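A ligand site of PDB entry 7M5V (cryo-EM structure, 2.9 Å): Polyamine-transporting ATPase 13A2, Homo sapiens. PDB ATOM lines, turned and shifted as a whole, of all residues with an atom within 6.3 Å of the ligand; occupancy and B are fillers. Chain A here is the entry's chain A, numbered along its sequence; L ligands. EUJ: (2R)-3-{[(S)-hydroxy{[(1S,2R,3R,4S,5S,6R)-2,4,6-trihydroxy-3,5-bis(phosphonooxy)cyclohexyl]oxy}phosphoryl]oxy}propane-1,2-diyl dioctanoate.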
ATOM      1  N   LYS A 420      -6.081  -4.644  -7.806  1.00  0.00           N
ATOM      2  CA  LYS A 420      -7.016  -3.533  -7.907  1.00  0.00           C
ATOM      3  C   LYS A 420      -7.562  -3.430  -9.322  1.00  0.00           C
ATOM      4  O   LYS A 420      -6.855  -3.696 -10.299  1.00  0.00           O
ATOM      5  CB  LYS A 420      -6.322  -2.230  -7.498  1.00  0.00           C
ATOM      6  CG  LYS A 420      -5.154  -1.753  -8.381  1.00  0.00           C
ATOM      7  CD  LYS A 420      -5.580  -0.834  -9.525  1.00  0.00           C
ATOM      8  CE  LYS A 420      -4.387  -0.313 -10.298  1.00  0.00           C
ATOM      9  NZ  LYS A 420      -4.792   0.571 -11.432  1.00  0.00           N
ATOM     10  N   PHE A 421      -8.836  -3.047  -9.427  1.00  0.00           N
ATOM     11  CA  PHE A 421      -9.473  -2.839 -10.721  1.00  0.00           C
ATOM     12  C   PHE A 421      -9.425  -1.370 -11.118  1.00  0.00           C
ATOM     13  O   PHE A 421      -8.987  -1.043 -12.232  1.00  0.00           O
ATOM     14  CB  PHE A 421     -10.939  -3.294 -10.664  1.00  0.00           C
ATOM     15  CG  PHE A 421     -11.139  -4.793 -10.626  1.00  0.00           C
ATOM     16  CD1 PHE A 421     -10.123  -5.687 -10.961  1.00  0.00           C
ATOM     17  CD2 PHE A 421     -12.365  -5.314 -10.239  1.00  0.00           C
ATOM     18  CE1 PHE A 421     -10.339  -7.049 -10.908  1.00  0.00           C
ATOM     19  CE2 PHE A 421     -12.579  -6.678 -10.197  1.00  0.00           C
ATOM     20  CZ  PHE A 421     -11.561  -7.547 -10.525  1.00  0.00           C
ATOM     21  N   TYR A 422      -9.866  -0.475 -10.235  1.00  0.00           N
ATOM     22  CA  TYR A 422      -9.672   0.960 -10.406  1.00  0.00           C
ATOM     23  C   TYR A 422      -8.793   1.546  -9.299  1.00  0.00           C
ATOM     24  O   TYR A 422      -7.713   2.062  -9.597  1.00  0.00           O
ATOM     25  CB  TYR A 422     -11.030   1.666 -10.436  1.00  0.00           C
ATOM     26  CG  TYR A 422     -11.950   1.121 -11.495  1.00  0.00           C
ATOM     27  CD1 TYR A 422     -11.884   1.577 -12.807  1.00  0.00           C
ATOM     28  CD2 TYR A 422     -12.895   0.143 -11.199  1.00  0.00           C
ATOM     29  CE1 TYR A 422     -12.726   1.087 -13.779  1.00  0.00           C
ATOM     30  CE2 TYR A 422     -13.731  -0.366 -12.168  1.00  0.00           C
ATOM     31  CZ  TYR A 422     -13.643   0.113 -13.459  1.00  0.00           C
ATOM     32  OH  TYR A 422     -14.472  -0.384 -14.428  1.00  0.00           O
ATOM     33  N   HIS A 424      -8.769   4.188  -8.050  1.00  0.00           N
ATOM     34  CA  HIS A 424      -8.443   5.559  -8.363  1.00  0.00           C
ATOM     35  C   HIS A 424      -9.673   6.389  -8.681  1.00  0.00           C
ATOM     36  O   HIS A 424      -9.530   7.564  -9.043  1.00  0.00           O
ATOM     37  CB  HIS A 424      -7.469   5.609  -9.545  1.00  0.00           C
ATOM     38  CG  HIS A 424      -6.605   6.835  -9.578  1.00  0.00           C
ATOM     39  ND1 HIS A 424      -7.007   8.009 -10.186  1.00  0.00           N
ATOM     40  CD2 HIS A 424      -5.370   7.065  -9.070  1.00  0.00           C
ATOM     41  CE1 HIS A 424      -6.042   8.909 -10.043  1.00  0.00           C
ATOM     42  NE2 HIS A 424      -5.050   8.359  -9.382  1.00  0.00           N
ATOM     43  N   LYS A 427     -10.328  10.116  -7.001  1.00  0.00           N
ATOM     44  CA  LYS A 427      -9.836  11.326  -7.639  1.00  0.00           C
ATOM     45  C   LYS A 427     -10.659  11.685  -8.867  1.00  0.00           C
ATOM     46  O   LYS A 427     -10.888  12.868  -9.149  1.00  0.00           O
ATOM     47  CB  LYS A 427      -8.363  11.167  -8.012  1.00  0.00           C
ATOM     48  CG  LYS A 427      -7.424  11.169  -6.816  1.00  0.00           C
ATOM     49  CD  LYS A 427      -6.100  10.499  -7.158  1.00  0.00           C
ATOM     50  CE  LYS A 427      -5.072  10.710  -6.064  1.00  0.00           C
ATOM     51  NZ  LYS A 427      -3.803   9.968  -6.362  1.00  0.00           N
ATOM     52  N   LYS A 506      -6.934  -8.916 -17.308  1.00  0.00           N
ATOM     53  CA  LYS A 506      -5.599  -8.462 -16.945  1.00  0.00           C
ATOM     54  C   LYS A 506      -4.736  -9.614 -16.449  1.00  0.00           C
ATOM     55  O   LYS A 506      -3.899  -9.432 -15.558  1.00  0.00           O
ATOM     56  CB  LYS A 506      -5.674  -7.359 -15.881  1.00  0.00           C
ATOM     57  CG  LYS A 506      -6.555  -7.688 -14.688  1.00  0.00           C
ATOM     58  CD  LYS A 506      -6.482  -6.614 -13.625  1.00  0.00           C
ATOM     59  CE  LYS A 506      -7.272  -5.364 -14.023  1.00  0.00           C
ATOM     60  NZ  LYS A 506      -7.120  -4.281 -13.030  1.00  0.00           N
ATOM     61  N   ARG A 991      -3.002  -4.309 -23.604  1.00  0.00           N
ATOM     62  CA  ARG A 991      -3.855  -4.578 -22.467  1.00  0.00           C
ATOM     63  C   ARG A 991      -4.806  -3.400 -22.242  1.00  0.00           C
ATOM     64  O   ARG A 991      -4.490  -2.267 -22.599  1.00  0.00           O
ATOM     65  CB  ARG A 991      -3.023  -4.811 -21.218  1.00  0.00           C
ATOM     66  CG  ARG A 991      -1.935  -5.853 -21.361  1.00  0.00           C
ATOM     67  CD  ARG A 991      -1.108  -5.955 -20.094  1.00  0.00           C
ATOM     68  NE  ARG A 991      -1.894  -6.419 -18.964  1.00  0.00           N
ATOM     69  CZ  ARG A 991      -1.483  -6.416 -17.703  1.00  0.00           C
ATOM     70  NH1 ARG A 991      -0.285  -5.957 -17.364  1.00  0.00           N
ATOM     71  NH2 ARG A 991      -2.288  -6.885 -16.761  1.00  0.00           N
ATOM     72  N   PRO A 992      -5.980  -3.641 -21.637  1.00  0.00           N
ATOM     73  CA  PRO A 992      -6.883  -2.531 -21.352  1.00  0.00           C
ATOM     74  C   PRO A 992      -6.307  -1.638 -20.266  1.00  0.00           C
ATOM     75  O   PRO A 992      -5.458  -2.087 -19.481  1.00  0.00           O
ATOM     76  CB  PRO A 992      -8.164  -3.232 -20.882  1.00  0.00           C
ATOM     77  CG  PRO A 992      -7.706  -4.521 -20.338  1.00  0.00           C
ATOM     78  CD  PRO A 992      -6.514  -4.922 -21.159  1.00  0.00           C
ATOM     79  N   PRO A 993      -6.740  -0.381 -20.173  1.00  0.00           N
ATOM     80  CA  PRO A 993      -6.259   0.482 -19.088  1.00  0.00           C
ATOM     81  C   PRO A 993      -6.668  -0.072 -17.736  1.00  0.00           C
ATOM     82  O   PRO A 993      -7.430  -1.032 -17.617  1.00  0.00           O
ATOM     83  CB  PRO A 993      -6.906   1.835 -19.366  1.00  0.00           C
ATOM     84  CG  PRO A 993      -7.379   1.781 -20.773  1.00  0.00           C
ATOM     85  CD  PRO A 993      -7.668   0.340 -21.069  1.00  0.00           C
ATOM     86  N   GLY A 994      -6.139   0.563 -16.686  1.00  0.00           N
ATOM     87  CA  GLY A 994      -6.423   0.170 -15.319  1.00  0.00           C
ATOM     88  C   GLY A 994      -6.826   1.326 -14.422  1.00  0.00           C
ATOM     89  O   GLY A 994      -6.994   1.146 -13.217  1.00  0.00           O
ATOM     90  N   ALA A 995      -6.992   2.515 -15.003  1.00  0.00           N
ATOM     91  CA  ALA A 995      -7.378   3.692 -14.230  1.00  0.00           C
ATOM     92  C   ALA A 995      -8.278   4.569 -15.087  1.00  0.00           C
ATOM     93  O   ALA A 995      -8.005   4.776 -16.269  1.00  0.00           O
ATOM     94  CB  ALA A 995      -6.156   4.478 -13.758  1.00  0.00           C
ATOM     95  N   LEU A 997      -8.678   7.796 -14.564  1.00  0.00           N
ATOM     96  CA  LEU A 997      -8.082   9.115 -14.669  1.00  0.00           C
ATOM     97  C   LEU A 997      -6.798   9.130 -15.483  1.00  0.00           C
ATOM     98  O   LEU A 997      -5.936   9.994 -15.260  1.00  0.00           O
ATOM     99  CB  LEU A 997      -7.824   9.689 -13.273  1.00  0.00           C
ATOM    100  CG  LEU A 997      -7.746  11.216 -13.161  1.00  0.00           C
ATOM    101  CD1 LEU A 997      -9.098  11.864 -13.458  1.00  0.00           C
ATOM    102  CD2 LEU A 997      -7.235  11.647 -11.802  1.00  0.00           C
ATOM    103  N   SER A 998      -6.636   8.200 -16.418  1.00  0.00           N
ATOM    104  CA  SER A 998      -5.485   8.254 -17.304  1.00  0.00           C
ATOM    105  C   SER A 998      -5.529   9.543 -18.138  1.00  0.00           C
ATOM    106  O   SER A 998      -6.561  10.216 -18.241  1.00  0.00           O
ATOM    107  CB  SER A 998      -5.461   7.037 -18.233  1.00  0.00           C
ATOM    108  OG  SER A 998      -6.491   7.102 -19.189  1.00  0.00           O
ATOM    109  N   VAL A 999      -4.380   9.880 -18.712  1.00  0.00           N
ATOM    110  CA  VAL A 999      -4.317  11.053 -19.591  1.00  0.00           C
ATOM    111  C   VAL A 999      -5.275  10.943 -20.761  1.00  0.00           C
ATOM    112  O   VAL A 999      -6.037  11.897 -20.990  1.00  0.00           O
ATOM    113  CB  VAL A 999      -2.860  11.288 -20.044  1.00  0.00           C
ATOM    114  CG1 VAL A 999      -2.803  12.333 -21.149  1.00  0.00           C
ATOM    115  CG2 VAL A 999      -1.996  11.704 -18.859  1.00  0.00           C
ATOM    116  N   ARG A1150       7.051  11.293 -21.720  1.00  0.00           N
ATOM    117  CA  ARG A1150       7.308  10.859 -20.328  1.00  0.00           C
ATOM    118  C   ARG A1150       7.856   9.428 -20.352  1.00  0.00           C
ATOM    119  O   ARG A1150       7.033   8.498 -20.444  1.00  0.00           O
ATOM    120  CB  ARG A1150       6.032  10.938 -19.487  1.00  0.00           C
ATOM    121  CG  ARG A1150       6.229  10.655 -18.007  1.00  0.00           C
ATOM    122  CD  ARG A1150       5.561   9.382 -17.500  1.00  0.00           C
ATOM    123  NE  ARG A1150       4.124   9.345 -17.725  1.00  0.00           N
ATOM    124  CZ  ARG A1150       3.299   8.366 -17.358  1.00  0.00           C
ATOM    125  NH1 ARG A1150       3.745   7.300 -16.710  1.00  0.00           N
ATOM    126  NH2 ARG A1150       2.004   8.458 -17.632  1.00  0.00           N
ATOM    127  N   LYS A1152       8.781   6.599 -18.581  1.00  0.00           N
ATOM    128  CA  LYS A1152       8.618   6.261 -17.132  1.00  0.00           C
ATOM    129  C   LYS A1152       9.678   5.247 -16.729  1.00  0.00           C
ATOM    130  O   LYS A1152      10.409   5.530 -15.760  1.00  0.00           O
ATOM    131  CB  LYS A1152       7.228   5.691 -16.836  1.00  0.00           C
ATOM    132  CG  LYS A1152       6.894   5.596 -15.354  1.00  0.00           C
ATOM    133  CD  LYS A1152       5.622   4.830 -15.047  1.00  0.00           C
ATOM    134  CE  LYS A1152       4.923   5.368 -13.816  1.00  0.00           C
ATOM    135  NZ  LYS A1152       3.775   4.520 -13.422  1.00  0.00           N
ATOM    136  N   ALA A1154       8.582   1.539 -16.167  1.00  0.00           N
ATOM    137  CA  ALA A1154       7.709   1.068 -15.092  1.00  0.00           C
ATOM    138  C   ALA A1154       8.432   0.053 -14.221  1.00  0.00           C
ATOM    139  O   ALA A1154       9.076  -0.876 -14.725  1.00  0.00           O
ATOM    140  CB  ALA A1154       6.438   0.467 -15.676  1.00  0.00           C
ATOM    141  N   SER A1155       8.319   0.237 -12.903  1.00  0.00           N
ATOM    142  CA  SER A1155       8.969  -0.653 -11.943  1.00  0.00           C
ATOM    143  C   SER A1155       8.068  -0.956 -10.747  1.00  0.00           C
ATOM    144  O   SER A1155       8.572  -1.436  -9.716  1.00  0.00           O
ATOM    145  CB  SER A1155      10.284  -0.058 -11.453  1.00  0.00           C
ATOM    146  OG  SER A1155      10.062   1.048 -10.600  1.00  0.00           O
ATOM    147  N   LYS A1156       6.767  -0.685 -10.837  1.00  0.00           N
ATOM    148  CA  LYS A1156       5.885  -0.956  -9.715  1.00  0.00           C
ATOM    149  C   LYS A1156       5.822  -2.447  -9.399  1.00  0.00           C
ATOM    150  O   LYS A1156       5.824  -2.839  -8.232  1.00  0.00           O
ATOM    151  CB  LYS A1156       4.486  -0.419 -10.012  1.00  0.00           C
ATOM    152  N   LYS A1157       5.791  -3.277 -10.435  1.00  0.00           N
ATOM    153  CA  LYS A1157       5.708  -4.723 -10.274  1.00  0.00           C
ATOM    154  C   LYS A1157       7.099  -5.322 -10.195  1.00  0.00           C
ATOM    155  O   LYS A1157       7.979  -4.966 -10.982  1.00  0.00           O
ATOM    156  CB  LYS A1157       4.922  -5.353 -11.419  1.00  0.00           C
ATOM    157  CG  LYS A1157       3.461  -4.932 -11.480  1.00  0.00           C
ATOM    158  CD  LYS A1157       2.967  -4.883 -12.918  1.00  0.00           C
ATOM    159  CE  LYS A1157       1.496  -4.497 -12.974  1.00  0.00           C
ATOM    160  NZ  LYS A1157       1.045  -4.242 -14.369  1.00  0.00           N
ATOM    161  N   LYS A1160       8.512  -7.300 -13.403  1.00  0.00           N
ATOM    162  CA  LYS A1160       9.042  -6.475 -14.473  1.00  0.00           C
ATOM    163  C   LYS A1160      10.453  -5.983 -14.145  1.00  0.00           C
ATOM    164  O   LYS A1160      11.316  -5.922 -15.029  1.00  0.00           O
ATOM    165  CB  LYS A1160       8.104  -5.297 -14.750  1.00  0.00           C
ATOM    166  CG  LYS A1160       6.777  -5.727 -15.352  1.00  0.00           C
ATOM    167  CD  LYS A1160       6.100  -4.598 -16.111  1.00  0.00           C
ATOM    168  CE  LYS A1160       4.955  -5.111 -16.957  1.00  0.00           C
ATOM    169  NZ  LYS A1160       4.007  -4.026 -17.343  1.00  0.00           N
HETATM  170  C1  EUJ L   1       1.104   2.191 -13.556  1.00  0.00           C
HETATM  171  C2  EUJ L   1       1.950   1.293 -14.443  1.00  0.00           C
HETATM  172  C3  EUJ L   1       2.013  -0.118 -13.893  1.00  0.00           C
HETATM  173  C4  EUJ L   1       0.626  -0.723 -13.899  1.00  0.00           C
HETATM  174  C5  EUJ L   1      -0.306   0.079 -12.990  1.00  0.00           C
HETATM  175  C6  EUJ L   1      -0.222   1.595 -13.080  1.00  0.00           C
HETATM  176  O1  EUJ L   1       0.749   3.305 -14.402  1.00  0.00           O
HETATM  177  O2  EUJ L   1       1.377   1.283 -15.751  1.00  0.00           O
HETATM  178  O3  EUJ L   1       2.949  -0.935 -14.686  1.00  0.00           O
HETATM  179  O4  EUJ L   1       0.103  -0.777 -15.233  1.00  0.00           O
HETATM  180  O5  EUJ L   1      -1.695  -0.250 -13.342  1.00  0.00           O
HETATM  181  O6  EUJ L   1      -0.502   2.128 -11.789  1.00  0.00           O
HETATM  182  P1  EUJ L   1      -0.042   4.537 -13.779  1.00  0.00           P
HETATM  183  O11 EUJ L   1       0.177   4.594 -12.292  1.00  0.00           O
HETATM  184  O12 EUJ L   1      -1.418   4.661 -14.371  1.00  0.00           O
HETATM  185  O13 EUJ L   1       0.979   5.578 -14.474  1.00  0.00           O
HETATM  186  P3  EUJ L   1       3.394  -0.858 -16.259  1.00  0.00           P
HETATM  187  O31 EUJ L   1       4.694  -1.644 -16.318  1.00  0.00           O
HETATM  188  O32 EUJ L   1       2.280  -1.511 -17.055  1.00  0.00           O
HETATM  189  O33 EUJ L   1       3.609   0.588 -16.655  1.00  0.00           O
HETATM  190  P5  EUJ L   1      -2.598   0.580 -14.407  1.00  0.00           P
HETATM  191  O51 EUJ L   1      -3.318   1.744 -13.750  1.00  0.00           O
HETATM  192  O52 EUJ L   1      -3.540  -0.523 -14.819  1.00  0.00           O
HETATM  193  O53 EUJ L   1      -1.730   1.029 -15.572  1.00  0.00           O
HETATM  194  C1A EUJ L   1       1.305   9.896 -14.633  1.00  0.00           C
HETATM  195  C1B EUJ L   1      -2.483   9.391 -12.324  1.00  0.00           C
HETATM  196  C1C EUJ L   1       1.284   6.881 -13.905  1.00  0.00           C
HETATM  197  C2A EUJ L   1       0.625  11.206 -14.385  1.00  0.00           C
HETATM  198  C2B EUJ L   1      -2.316  10.829 -11.966  1.00  0.00           C
HETATM  199  C2C EUJ L   1       0.114   7.790 -14.247  1.00  0.00           C
HETATM  200  C3A EUJ L   1       1.034  11.874 -13.114  1.00  0.00           C
HETATM  201  C3B EUJ L   1      -2.920  11.182 -10.647  1.00  0.00           C
HETATM  202  C3C EUJ L   1      -0.585   8.297 -13.011  1.00  0.00           C
HETATM  203  C4A EUJ L   1       0.284  13.180 -12.887  1.00  0.00           C
HETATM  204  C4B EUJ L   1      -2.783  12.650 -10.309  1.00  0.00           C
HETATM  205  C5A EUJ L   1       0.458  14.221 -13.982  1.00  0.00           C
HETATM  206  C5B EUJ L   1      -3.795  13.519 -10.998  1.00  0.00           C
HETATM  207  C6A EUJ L   1       0.296  15.604 -13.464  1.00  0.00           C
HETATM  208  C6B EUJ L   1      -3.810  14.956 -10.537  1.00  0.00           C
HETATM  209  C7A EUJ L   1       0.010  16.635 -14.490  1.00  0.00           C
HETATM  210  C7B EUJ L   1      -3.120  15.927 -11.471  1.00  0.00           C
HETATM  211  C8A EUJ L   1      -0.379  17.923 -13.840  1.00  0.00           C
HETATM  212  C8B EUJ L   1      -3.418  17.364 -11.139  1.00  0.00           C
HETATM  213  O1A EUJ L   1       2.485   9.723 -14.508  1.00  0.00           O
HETATM  214  O1B EUJ L   1      -3.197   8.612 -11.746  1.00  0.00           O
HETATM  215  O2C EUJ L   1       0.485   8.925 -15.098  1.00  0.00           O
HETATM  216  O3C EUJ L   1      -1.755   9.053 -13.368  1.00  0.00           O
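The side-chain amino group (NZ) of Lys 1160 is in salt-bridge range of an oxygen (O31) of the ligand (2.7 Å).
An oxygen (O2C) of the ligand is in hydrogen-bond range of the guanidinium group (NH2) of Arg 1150 (3.0 Å).
NE2 of His 424 sits at hydrogen-bond distance from O1B of the ligand, 3.0 Å away.
NZ of Lys 1152 lies within salt-bridge range of O11 of the ligand.
The side-chain amino group of Lys 420 lies within salt-bridge range of an oxygen (O51) of the ligand.
N of Gly 994 lies close to O52 of the ligand, 3.4 Å away.
The side-chain amino group of Lys 420 lies within hydrogen-bond range of the backbone carbonyl oxygen of Gly 994, 2.9 Å away.
NZ of Lys 506 is in hydrogen-bond range of O of Lys 420 (2.8 Å).
Merely in contact with the ligand: Ala 1154, Lys 1157, Ala 995 and Leu 997.
Of the 21 residues printed, 10 come within 4 Å of the ligand.
The nearest printed residue that does not touch the ligand is Pro 993 (4.3 Å).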
